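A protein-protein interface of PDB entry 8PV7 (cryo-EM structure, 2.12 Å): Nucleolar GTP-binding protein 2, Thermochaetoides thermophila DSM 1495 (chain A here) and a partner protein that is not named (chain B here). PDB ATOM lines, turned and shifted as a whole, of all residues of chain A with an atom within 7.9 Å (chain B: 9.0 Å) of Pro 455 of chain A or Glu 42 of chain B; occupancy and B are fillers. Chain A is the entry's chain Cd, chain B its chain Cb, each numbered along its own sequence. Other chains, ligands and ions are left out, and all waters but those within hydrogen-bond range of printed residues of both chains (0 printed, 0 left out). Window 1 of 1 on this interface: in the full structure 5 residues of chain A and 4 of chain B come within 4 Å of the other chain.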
ATOM      1  N   ILE A 436       0.659  -5.707 -17.663  1.00  0.00           N
ATOM      2  CA  ILE A 436       0.871  -6.714 -18.700  1.00  0.00           C
ATOM      3  C   ILE A 436      -0.336  -6.788 -19.623  1.00  0.00           C
ATOM      4  O   ILE A 436      -0.201  -6.777 -20.853  1.00  0.00           O
ATOM      5  CB  ILE A 436       1.184  -8.081 -18.069  1.00  0.00           C
ATOM      6  CG1 ILE A 436       2.474  -8.007 -17.254  1.00  0.00           C
ATOM      7  CG2 ILE A 436       1.307  -9.146 -19.140  1.00  0.00           C
ATOM      8  CD1 ILE A 436       3.688  -7.659 -18.084  1.00  0.00           C
ATOM      9  N   LEU A 439      -0.537  -3.619 -21.804  1.00  0.00           N
ATOM     10  CA  LEU A 439       0.360  -3.668 -22.950  1.00  0.00           C
ATOM     11  C   LEU A 439      -0.132  -4.656 -24.001  1.00  0.00           C
ATOM     12  O   LEU A 439      -0.019  -4.393 -25.201  1.00  0.00           O
ATOM     13  CB  LEU A 439       1.775  -4.020 -22.495  1.00  0.00           C
ATOM     14  CG  LEU A 439       2.443  -2.952 -21.623  1.00  0.00           C
ATOM     15  CD1 LEU A 439       3.746  -3.447 -21.023  1.00  0.00           C
ATOM     16  CD2 LEU A 439       2.660  -1.664 -22.392  1.00  0.00           C
ATOM     17  N   GLU A 440      -0.706  -5.785 -23.570  1.00  0.00           N
ATOM     18  CA  GLU A 440      -1.200  -6.775 -24.524  1.00  0.00           C
ATOM     19  C   GLU A 440      -2.395  -6.253 -25.315  1.00  0.00           C
ATOM     20  O   GLU A 440      -2.460  -6.426 -26.537  1.00  0.00           O
ATOM     21  CB  GLU A 440      -1.559  -8.072 -23.802  1.00  0.00           C
ATOM     22  CG  GLU A 440      -0.356  -8.864 -23.336  1.00  0.00           C
ATOM     23  CD  GLU A 440      -0.736 -10.029 -22.447  1.00  0.00           C
ATOM     24  OE1 GLU A 440      -1.936 -10.176 -22.139  1.00  0.00           O
ATOM     25  OE2 GLU A 440       0.166 -10.792 -22.046  1.00  0.00           O
ATOM     26  N   MET A 441      -3.358  -5.618 -24.638  1.00  0.00           N
ATOM     27  CA  MET A 441      -4.506  -5.055 -25.347  1.00  0.00           C
ATOM     28  C   MET A 441      -4.093  -3.911 -26.263  1.00  0.00           C
ATOM     29  O   MET A 441      -4.620  -3.779 -27.373  1.00  0.00           O
ATOM     30  CB  MET A 441      -5.595  -4.605 -24.369  1.00  0.00           C
ATOM     31  CG  MET A 441      -6.045  -5.667 -23.385  1.00  0.00           C
ATOM     32  SD  MET A 441      -6.945  -5.021 -21.962  1.00  0.00           S
ATOM     33  CE  MET A 441      -7.922  -3.735 -22.719  1.00  0.00           C
ATOM     34  N   LEU A 442      -3.137  -3.082 -25.828  1.00  0.00           N
ATOM     35  CA  LEU A 442      -2.646  -2.029 -26.710  1.00  0.00           C
ATOM     36  C   LEU A 442      -1.939  -2.613 -27.933  1.00  0.00           C
ATOM     37  O   LEU A 442      -2.107  -2.109 -29.050  1.00  0.00           O
ATOM     38  CB  LEU A 442      -1.724  -1.084 -25.941  1.00  0.00           C
ATOM     39  CG  LEU A 442      -1.287   0.183 -26.682  1.00  0.00           C
ATOM     40  CD1 LEU A 442      -2.460   0.845 -27.384  1.00  0.00           C
ATOM     41  CD2 LEU A 442      -0.608   1.162 -25.741  1.00  0.00           C
ATOM     42  N   ALA A 443      -1.168  -3.686 -27.745  1.00  0.00           N
ATOM     43  CA  ALA A 443      -0.476  -4.321 -28.863  1.00  0.00           C
ATOM     44  C   ALA A 443      -1.452  -4.942 -29.852  1.00  0.00           C
ATOM     45  O   ALA A 443      -1.276  -4.815 -31.069  1.00  0.00           O
ATOM     46  CB  ALA A 443       0.496  -5.376 -28.345  1.00  0.00           C
ATOM     47  N   ARG A 444      -2.490  -5.614 -29.350  1.00  0.00           N
ATOM     48  CA  ARG A 444      -3.469  -6.222 -30.245  1.00  0.00           C
ATOM     49  C   ARG A 444      -4.296  -5.166 -30.961  1.00  0.00           C
ATOM     50  O   ARG A 444      -4.674  -5.351 -32.121  1.00  0.00           O
ATOM     51  CB  ARG A 444      -4.378  -7.177 -29.479  1.00  0.00           C
ATOM     52  CG  ARG A 444      -3.659  -8.356 -28.882  1.00  0.00           C
ATOM     53  CD  ARG A 444      -4.625  -9.435 -28.448  1.00  0.00           C
ATOM     54  NE  ARG A 444      -3.981 -10.380 -27.546  1.00  0.00           N
ATOM     55  CZ  ARG A 444      -4.042 -10.301 -26.225  1.00  0.00           C
ATOM     56  NH1 ARG A 444      -4.767  -9.373 -25.622  1.00  0.00           N
ATOM     57  NH2 ARG A 444      -3.357 -11.170 -25.490  1.00  0.00           N
ATOM     58  N   LYS A 445      -4.581  -4.048 -30.291  1.00  0.00           N
ATOM     59  CA  LYS A 445      -5.342  -2.987 -30.935  1.00  0.00           C
ATOM     60  C   LYS A 445      -4.520  -2.288 -32.010  1.00  0.00           C
ATOM     61  O   LYS A 445      -5.028  -2.005 -33.100  1.00  0.00           O
ATOM     62  CB  LYS A 445      -5.818  -1.986 -29.890  1.00  0.00           C
ATOM     63  CG  LYS A 445      -6.602  -0.846 -30.464  1.00  0.00           C
ATOM     64  CD  LYS A 445      -6.741   0.264 -29.463  1.00  0.00           C
ATOM     65  CE  LYS A 445      -7.355   1.477 -30.109  1.00  0.00           C
ATOM     66  NZ  LYS A 445      -7.303   2.631 -29.197  1.00  0.00           N
ATOM     67  N   GLY A 447      -1.925  -3.528 -33.597  1.00  0.00           N
ATOM     68  CA  GLY A 447      -1.322  -4.423 -34.561  1.00  0.00           C
ATOM     69  C   GLY A 447       0.151  -4.672 -34.352  1.00  0.00           C
ATOM     70  O   GLY A 447       0.838  -5.091 -35.282  1.00  0.00           O
ATOM     71  N   ARG A 448       0.660  -4.419 -33.149  1.00  0.00           N
ATOM     72  CA  ARG A 448       2.064  -4.662 -32.832  1.00  0.00           C
ATOM     73  C   ARG A 448       2.213  -6.136 -32.474  1.00  0.00           C
ATOM     74  O   ARG A 448       2.213  -6.540 -31.310  1.00  0.00           O
ATOM     75  CB  ARG A 448       2.524  -3.743 -31.711  1.00  0.00           C
ATOM     76  CG  ARG A 448       2.535  -2.266 -32.087  1.00  0.00           C
ATOM     77  CD  ARG A 448       3.816  -1.833 -32.801  1.00  0.00           C
ATOM     78  NE  ARG A 448       3.918  -2.317 -34.174  1.00  0.00           N
ATOM     79  CZ  ARG A 448       3.209  -1.866 -35.199  1.00  0.00           C
ATOM     80  NH1 ARG A 448       2.333  -0.885 -35.062  1.00  0.00           N
ATOM     81  NH2 ARG A 448       3.394  -2.406 -36.399  1.00  0.00           N
ATOM     82  N   LEU A 449       2.331  -6.956 -33.513  1.00  0.00           N
ATOM     83  CA  LEU A 449       2.340  -8.402 -33.380  1.00  0.00           C
ATOM     84  C   LEU A 449       3.636  -8.974 -33.931  1.00  0.00           C
ATOM     85  O   LEU A 449       4.179  -8.486 -34.926  1.00  0.00           O
ATOM     86  CB  LEU A 449       1.152  -9.031 -34.115  1.00  0.00           C
ATOM     87  CG  LEU A 449      -0.223  -8.411 -33.870  1.00  0.00           C
ATOM     88  CD1 LEU A 449      -1.232  -8.959 -34.864  1.00  0.00           C
ATOM     89  CD2 LEU A 449      -0.680  -8.668 -32.447  1.00  0.00           C
ATOM     90  N   LEU A 450       4.130 -10.008 -33.267  1.00  0.00           N
ATOM     91  CA  LEU A 450       5.272 -10.766 -33.745  1.00  0.00           C
ATOM     92  C   LEU A 450       4.771 -11.903 -34.635  1.00  0.00           C
ATOM     93  O   LEU A 450       3.607 -11.935 -35.037  1.00  0.00           O
ATOM     94  CB  LEU A 450       6.100 -11.257 -32.562  1.00  0.00           C
ATOM     95  CG  LEU A 450       6.617 -10.133 -31.663  1.00  0.00           C
ATOM     96  CD1 LEU A 450       7.339 -10.683 -30.449  1.00  0.00           C
ATOM     97  CD2 LEU A 450       7.520  -9.199 -32.450  1.00  0.00           C
ATOM     98  N   LYS A 451       5.655 -12.841 -34.972  1.00  0.00           N
ATOM     99  CA  LYS A 451       5.244 -14.009 -35.742  1.00  0.00           C
ATOM    100  C   LYS A 451       4.306 -14.880 -34.921  1.00  0.00           C
ATOM    101  O   LYS A 451       4.570 -15.166 -33.750  1.00  0.00           O
ATOM    102  CB  LYS A 451       6.466 -14.814 -36.175  1.00  0.00           C
ATOM    103  CG  LYS A 451       7.476 -14.022 -36.976  1.00  0.00           C
ATOM    104  CD  LYS A 451       6.842 -13.406 -38.207  1.00  0.00           C
ATOM    105  CE  LYS A 451       7.840 -12.530 -38.949  1.00  0.00           C
ATOM    106  NZ  LYS A 451       7.224 -11.852 -40.121  1.00  0.00           N
ATOM    107  N   GLY A 452       3.205 -15.292 -35.536  1.00  0.00           N
ATOM    108  CA  GLY A 452       2.183 -16.038 -34.841  1.00  0.00           C
ATOM    109  C   GLY A 452       1.178 -15.206 -34.081  1.00  0.00           C
ATOM    110  O   GLY A 452       0.497 -15.743 -33.204  1.00  0.00           O
ATOM    111  N   GLY A 453       1.083 -13.908 -34.359  1.00  0.00           N
ATOM    112  CA  GLY A 453       0.121 -13.070 -33.675  1.00  0.00           C
ATOM    113  C   GLY A 453       0.444 -12.764 -32.230  1.00  0.00           C
ATOM    114  O   GLY A 453      -0.420 -12.241 -31.519  1.00  0.00           O
ATOM    115  N   GLU A 454       1.647 -13.083 -31.773  1.00  0.00           N
ATOM    116  CA  GLU A 454       2.034 -12.800 -30.398  1.00  0.00           C
ATOM    117  C   GLU A 454       2.242 -11.300 -30.211  1.00  0.00           C
ATOM    118  O   GLU A 454       2.925 -10.672 -31.025  1.00  0.00           O
ATOM    119  CB  GLU A 454       3.306 -13.565 -30.049  1.00  0.00           C
ATOM    120  CG  GLU A 454       3.859 -13.260 -28.676  1.00  0.00           C
ATOM    121  CD  GLU A 454       5.323 -13.615 -28.551  1.00  0.00           C
ATOM    122  OE1 GLU A 454       5.924 -14.019 -29.568  1.00  0.00           O
ATOM    123  OE2 GLU A 454       5.876 -13.492 -27.440  1.00  0.00           O
ATOM    124  N   PRO A 455       1.668 -10.696 -29.170  1.00  0.00           N
ATOM    125  CA  PRO A 455       1.784  -9.240 -28.991  1.00  0.00           C
ATOM    126  C   PRO A 455       3.209  -8.792 -28.687  1.00  0.00           C
ATOM    127  O   PRO A 455       3.931  -9.429 -27.917  1.00  0.00           O
ATOM    128  CB  PRO A 455       0.842  -8.961 -27.816  1.00  0.00           C
ATOM    129  CG  PRO A 455       0.696 -10.261 -27.119  1.00  0.00           C
ATOM    130  CD  PRO A 455       0.762 -11.300 -28.182  1.00  0.00           C
ATOM    131  N   ASP A 456       3.604  -7.673 -29.299  1.00  0.00           N
ATOM    132  CA  ASP A 456       4.937  -7.092 -29.112  1.00  0.00           C
ATOM    133  C   ASP A 456       4.896  -6.173 -27.895  1.00  0.00           C
ATOM    134  O   ASP A 456       4.827  -4.942 -27.989  1.00  0.00           O
ATOM    135  CB  ASP A 456       5.385  -6.358 -30.368  1.00  0.00           C
ATOM    136  CG  ASP A 456       6.854  -5.985 -30.338  1.00  0.00           C
ATOM    137  OD1 ASP A 456       7.566  -6.403 -29.402  1.00  0.00           O
ATOM    138  OD2 ASP A 456       7.301  -5.281 -31.264  1.00  0.00           O
ATOM    139  N   VAL A 457       4.950  -6.809 -26.725  1.00  0.00           N
ATOM    140  CA  VAL A 457       4.846  -6.097 -25.458  1.00  0.00           C
ATOM    141  C   VAL A 457       6.063  -5.200 -25.241  1.00  0.00           C
ATOM    142  O   VAL A 457       5.940  -4.087 -24.719  1.00  0.00           O
ATOM    143  CB  VAL A 457       4.650  -7.121 -24.324  1.00  0.00           C
ATOM    144  CG1 VAL A 457       4.593  -6.451 -22.988  1.00  0.00           C
ATOM    145  CG2 VAL A 457       3.380  -7.915 -24.561  1.00  0.00           C
ATOM    146  N   ASP A 458       7.241  -5.651 -25.686  1.00  0.00           N
ATOM    147  CA  ASP A 458       8.460  -4.843 -25.610  1.00  0.00           C
ATOM    148  C   ASP A 458       8.333  -3.540 -26.397  1.00  0.00           C
ATOM    149  O   ASP A 458       8.598  -2.450 -25.868  1.00  0.00           O
ATOM    150  CB  ASP A 458       9.635  -5.660 -26.147  1.00  0.00           C
ATOM    151  CG  ASP A 458      10.942  -5.335 -25.466  1.00  0.00           C
ATOM    152  OD1 ASP A 458      11.712  -4.515 -26.011  1.00  0.00           O
ATOM    153  OD2 ASP A 458      11.225  -5.939 -24.412  1.00  0.00           O
ATOM    154  N   GLY A 459       7.923  -3.637 -27.664  1.00  0.00           N
ATOM    155  CA  GLY A 459       7.802  -2.448 -28.488  1.00  0.00           C
ATOM    156  C   GLY A 459       6.696  -1.520 -28.021  1.00  0.00           C
ATOM    157  O   GLY A 459       6.833  -0.294 -28.077  1.00  0.00           O
ATOM    158  N   VAL A 460       5.586  -2.093 -27.552  1.00  0.00           N
ATOM    159  CA  VAL A 460       4.492  -1.264 -27.054  1.00  0.00           C
ATOM    160  C   VAL A 460       4.911  -0.541 -25.777  1.00  0.00           C
ATOM    161  O   VAL A 460       4.562   0.628 -25.567  1.00  0.00           O
ATOM    162  CB  VAL A 460       3.227  -2.123 -26.872  1.00  0.00           C
ATOM    163  CG1 VAL A 460       2.176  -1.415 -26.041  1.00  0.00           C
ATOM    164  CG2 VAL A 460       2.660  -2.450 -28.224  1.00  0.00           C
ATOM    165  N   LYS B  36      -0.629 -28.918 -24.189  1.00  0.00           N
ATOM    166  CA  LYS B  36      -1.016 -27.514 -24.104  1.00  0.00           C
ATOM    167  C   LYS B  36      -0.466 -26.850 -22.849  1.00  0.00           C
ATOM    168  O   LYS B  36      -0.275 -25.629 -22.831  1.00  0.00           O
ATOM    169  CB  LYS B  36      -2.535 -27.382 -24.156  1.00  0.00           C
ATOM    170  CG  LYS B  36      -3.121 -27.679 -25.517  1.00  0.00           C
ATOM    171  CD  LYS B  36      -4.570 -27.250 -25.595  1.00  0.00           C
ATOM    172  CE  LYS B  36      -5.094 -27.367 -27.008  1.00  0.00           C
ATOM    173  NZ  LYS B  36      -6.494 -26.880 -27.115  1.00  0.00           N
ATOM    174  N   LYS B  39       2.842 -24.989 -23.197  1.00  0.00           N
ATOM    175  CA  LYS B  39       2.831 -23.721 -23.911  1.00  0.00           C
ATOM    176  C   LYS B  39       2.267 -22.619 -23.020  1.00  0.00           C
ATOM    177  O   LYS B  39       1.755 -22.877 -21.927  1.00  0.00           O
ATOM    178  CB  LYS B  39       2.005 -23.808 -25.201  1.00  0.00           C
ATOM    179  CG  LYS B  39       2.827 -23.960 -26.468  1.00  0.00           C
ATOM    180  CD  LYS B  39       3.283 -25.395 -26.655  1.00  0.00           C
ATOM    181  CE  LYS B  39       4.444 -25.476 -27.627  1.00  0.00           C
ATOM    182  NZ  LYS B  39       4.105 -24.883 -28.946  1.00  0.00           N
ATOM    183  N   ALA B  40       2.365 -21.382 -23.501  1.00  0.00           N
ATOM    184  CA  ALA B  40       1.835 -20.212 -22.811  1.00  0.00           C
ATOM    185  C   ALA B  40       0.654 -19.668 -23.601  1.00  0.00           C
ATOM    186  O   ALA B  40       0.777 -19.407 -24.802  1.00  0.00           O
ATOM    187  CB  ALA B  40       2.909 -19.138 -22.642  1.00  0.00           C
ATOM    188  N   ALA B  41      -0.480 -19.480 -22.922  1.00  0.00           N
ATOM    189  CA  ALA B  41      -1.726 -19.170 -23.619  1.00  0.00           C
ATOM    190  C   ALA B  41      -1.726 -17.755 -24.184  1.00  0.00           C
ATOM    191  O   ALA B  41      -2.356 -17.493 -25.214  1.00  0.00           O
ATOM    192  CB  ALA B  41      -2.914 -19.369 -22.680  1.00  0.00           C
ATOM    193  N   GLU B  42      -1.037 -16.826 -23.520  1.00  0.00           N
ATOM    194  CA  GLU B  42      -1.042 -15.440 -23.972  1.00  0.00           C
ATOM    195  C   GLU B  42      -0.177 -15.226 -25.208  1.00  0.00           C
ATOM    196  O   GLU B  42      -0.342 -14.210 -25.892  1.00  0.00           O
ATOM    197  CB  GLU B  42      -0.581 -14.514 -22.843  1.00  0.00           C
ATOM    198  CG  GLU B  42       0.770 -14.871 -22.238  1.00  0.00           C
ATOM    199  CD  GLU B  42       0.654 -15.786 -21.034  1.00  0.00           C
ATOM    200  OE1 GLU B  42      -0.436 -16.356 -20.818  1.00  0.00           O
ATOM    201  OE2 GLU B  42       1.654 -15.930 -20.301  1.00  0.00           O
ATOM    202  N   ASP B  43       0.733 -16.146 -25.508  1.00  0.00           N
ATOM    203  CA  ASP B  43       1.578 -16.052 -26.691  1.00  0.00           C
ATOM    204  C   ASP B  43       1.019 -16.809 -27.888  1.00  0.00           C
ATOM    205  O   ASP B  43       1.663 -16.830 -28.941  1.00  0.00           O
ATOM    206  CB  ASP B  43       2.983 -16.570 -26.374  1.00  0.00           C
ATOM    207  CG  ASP B  43       3.694 -15.726 -25.342  1.00  0.00           C
ATOM    208  OD1 ASP B  43       4.933 -15.841 -25.231  1.00  0.00           O
ATOM    209  OD2 ASP B  43       3.019 -14.942 -24.648  1.00  0.00           O
ATOM    210  N   LEU B  44      -0.131 -17.424 -27.756  1.00  0.00           N
ATOM    211  CA  LEU B  44      -0.721 -18.221 -28.816  1.00  0.00           C
ATOM    212  C   LEU B  44      -1.659 -17.374 -29.668  1.00  0.00           C
ATOM    213  O   LEU B  44      -2.206 -16.378 -29.189  1.00  0.00           O
ATOM    214  CB  LEU B  44      -1.492 -19.406 -28.226  1.00  0.00           C
ATOM    215  CG  LEU B  44      -0.620 -20.485 -27.590  1.00  0.00           C
ATOM    216  CD1 LEU B  44      -1.474 -21.545 -26.930  1.00  0.00           C
ATOM    217  CD2 LEU B  44       0.309 -21.100 -28.621  1.00  0.00           C
ATOM    218  N   PRO B  45      -1.834 -17.733 -30.941  1.00  0.00           N
ATOM    219  CA  PRO B  45      -2.833 -17.051 -31.772  1.00  0.00           C
ATOM    220  C   PRO B  45      -4.236 -17.212 -31.205  1.00  0.00           C
ATOM    221  O   PRO B  45      -4.650 -18.310 -30.827  1.00  0.00           O
ATOM    222  CB  PRO B  45      -2.697 -17.748 -33.129  1.00  0.00           C
ATOM    223  CG  PRO B  45      -1.349 -18.340 -33.133  1.00  0.00           C
ATOM    224  CD  PRO B  45      -1.004 -18.667 -31.721  1.00  0.00           C
ATOM    225  N   GLY B  46      -4.967 -16.102 -31.149  1.00  0.00           N
ATOM    226  CA  GLY B  46      -6.318 -16.109 -30.620  1.00  0.00           C
ATOM    227  C   GLY B  46      -6.428 -16.502 -29.167  1.00  0.00           C
ATOM    228  O   GLY B  46      -7.473 -17.012 -28.754  1.00  0.00           O
ATOM    229  N   LEU B  47      -5.366 -16.288 -28.383  1.00  0.00           N
ATOM    230  CA  LEU B  47      -5.253 -16.699 -26.982  1.00  0.00           C
ATOM    231  C   LEU B  47      -5.443 -18.200 -26.794  1.00  0.00           C
ATOM    232  O   LEU B  47      -5.892 -18.641 -25.733  1.00  0.00           O
ATOM    233  CB  LEU B  47      -6.222 -15.931 -26.069  1.00  0.00           C
ATOM    234  CG  LEU B  47      -5.949 -14.460 -25.735  1.00  0.00           C
ATOM    235  CD1 LEU B  47      -4.514 -14.310 -25.260  1.00  0.00           C
ATOM    236  CD2 LEU B  47      -6.267 -13.495 -26.871  1.00  0.00           C
ATOM    237  N   GLY B  48      -5.108 -18.996 -27.805  1.00  0.00           N
ATOM    238  CA  GLY B  48      -5.236 -20.434 -27.728  1.00  0.00           C
ATOM    239  C   GLY B  48      -6.643 -20.969 -27.859  1.00  0.00           C
ATOM    240  O   GLY B  48      -6.845 -22.172 -27.667  1.00  0.00           O
ATOM    241  N   LEU B  49      -7.619 -20.124 -28.184  1.00  0.00           N
ATOM    242  CA  LEU B  49      -9.008 -20.561 -28.214  1.00  0.00           C
ATOM    243  C   LEU B  49      -9.370 -21.347 -29.467  1.00  0.00           C
ATOM    244  O   LEU B  49     -10.382 -22.052 -29.461  1.00  0.00           O
ATOM    245  CB  LEU B  49      -9.938 -19.355 -28.091  1.00  0.00           C
ATOM    246  CG  LEU B  49      -9.894 -18.629 -26.748  1.00  0.00           C
ATOM    247  CD1 LEU B  49     -10.839 -17.447 -26.752  1.00  0.00           C
ATOM    248  CD2 LEU B  49     -10.227 -19.582 -25.617  1.00  0.00           C
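The side-chain carboxylate (OE1) of Glu 440 of chain A lies within salt-bridge range of the guanidinium group (NH2) of Arg 444 of chain A (3.8 Å).
OE2 of Glu 454 of chain A lies close to OD1 of Asp 43 of chain B, 3.4 Å away.
Of chain B, only Glu 42 (3.9 Å) comes within 4 Å of Pro 455 of chain A. Glu 42 of chain B touches two residues of chain A. Printed residues of chain A within 4 Å of Pro 45 of chain B: Gly 452 (3.2 Å). Printed residues of chain B within 4 Å of Gly 452 of chain A: Pro 45. Printed residues of chain B within 4 Å of Arg 444 of chain A: Leu 47. Leu 439 of chain A touches none of the printed residues of chain B. The nearest residue of chain B that does not touch Pro 455 of chain A is Asp 43 of chain B (5.0 Å). The nearest printed residue of chain B that does not touch Glu 440 of chain A is Asp 43 of chain B (5.7 Å).
Glu 440 of chain A touches Glu 42 of chain B (OE2 to CB, 3.9 Å). NH2 of Arg 444 of chain A touches CD1 of Leu 47 of chain B, at 3.4 Å. Gly 452 of chain A touches Pro 45 of chain B (O to CG, 3.2 Å). CD of Pro 455 of chain A touches O of Glu 42 of chain B, 3.9 Å away.
Of the 22 printed residues of chain A, 5 touch a printed residue of chain B. Along chain B the printed residues that touch a printed residue of chain A span positions 42 to 47. Among the printed residues, 5 pairs touch across the chains. Among the printed residues, no Asp or Glu carboxylate lies within 4 Å of a Lys or Arg side-chain nitrogen of the other chain.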
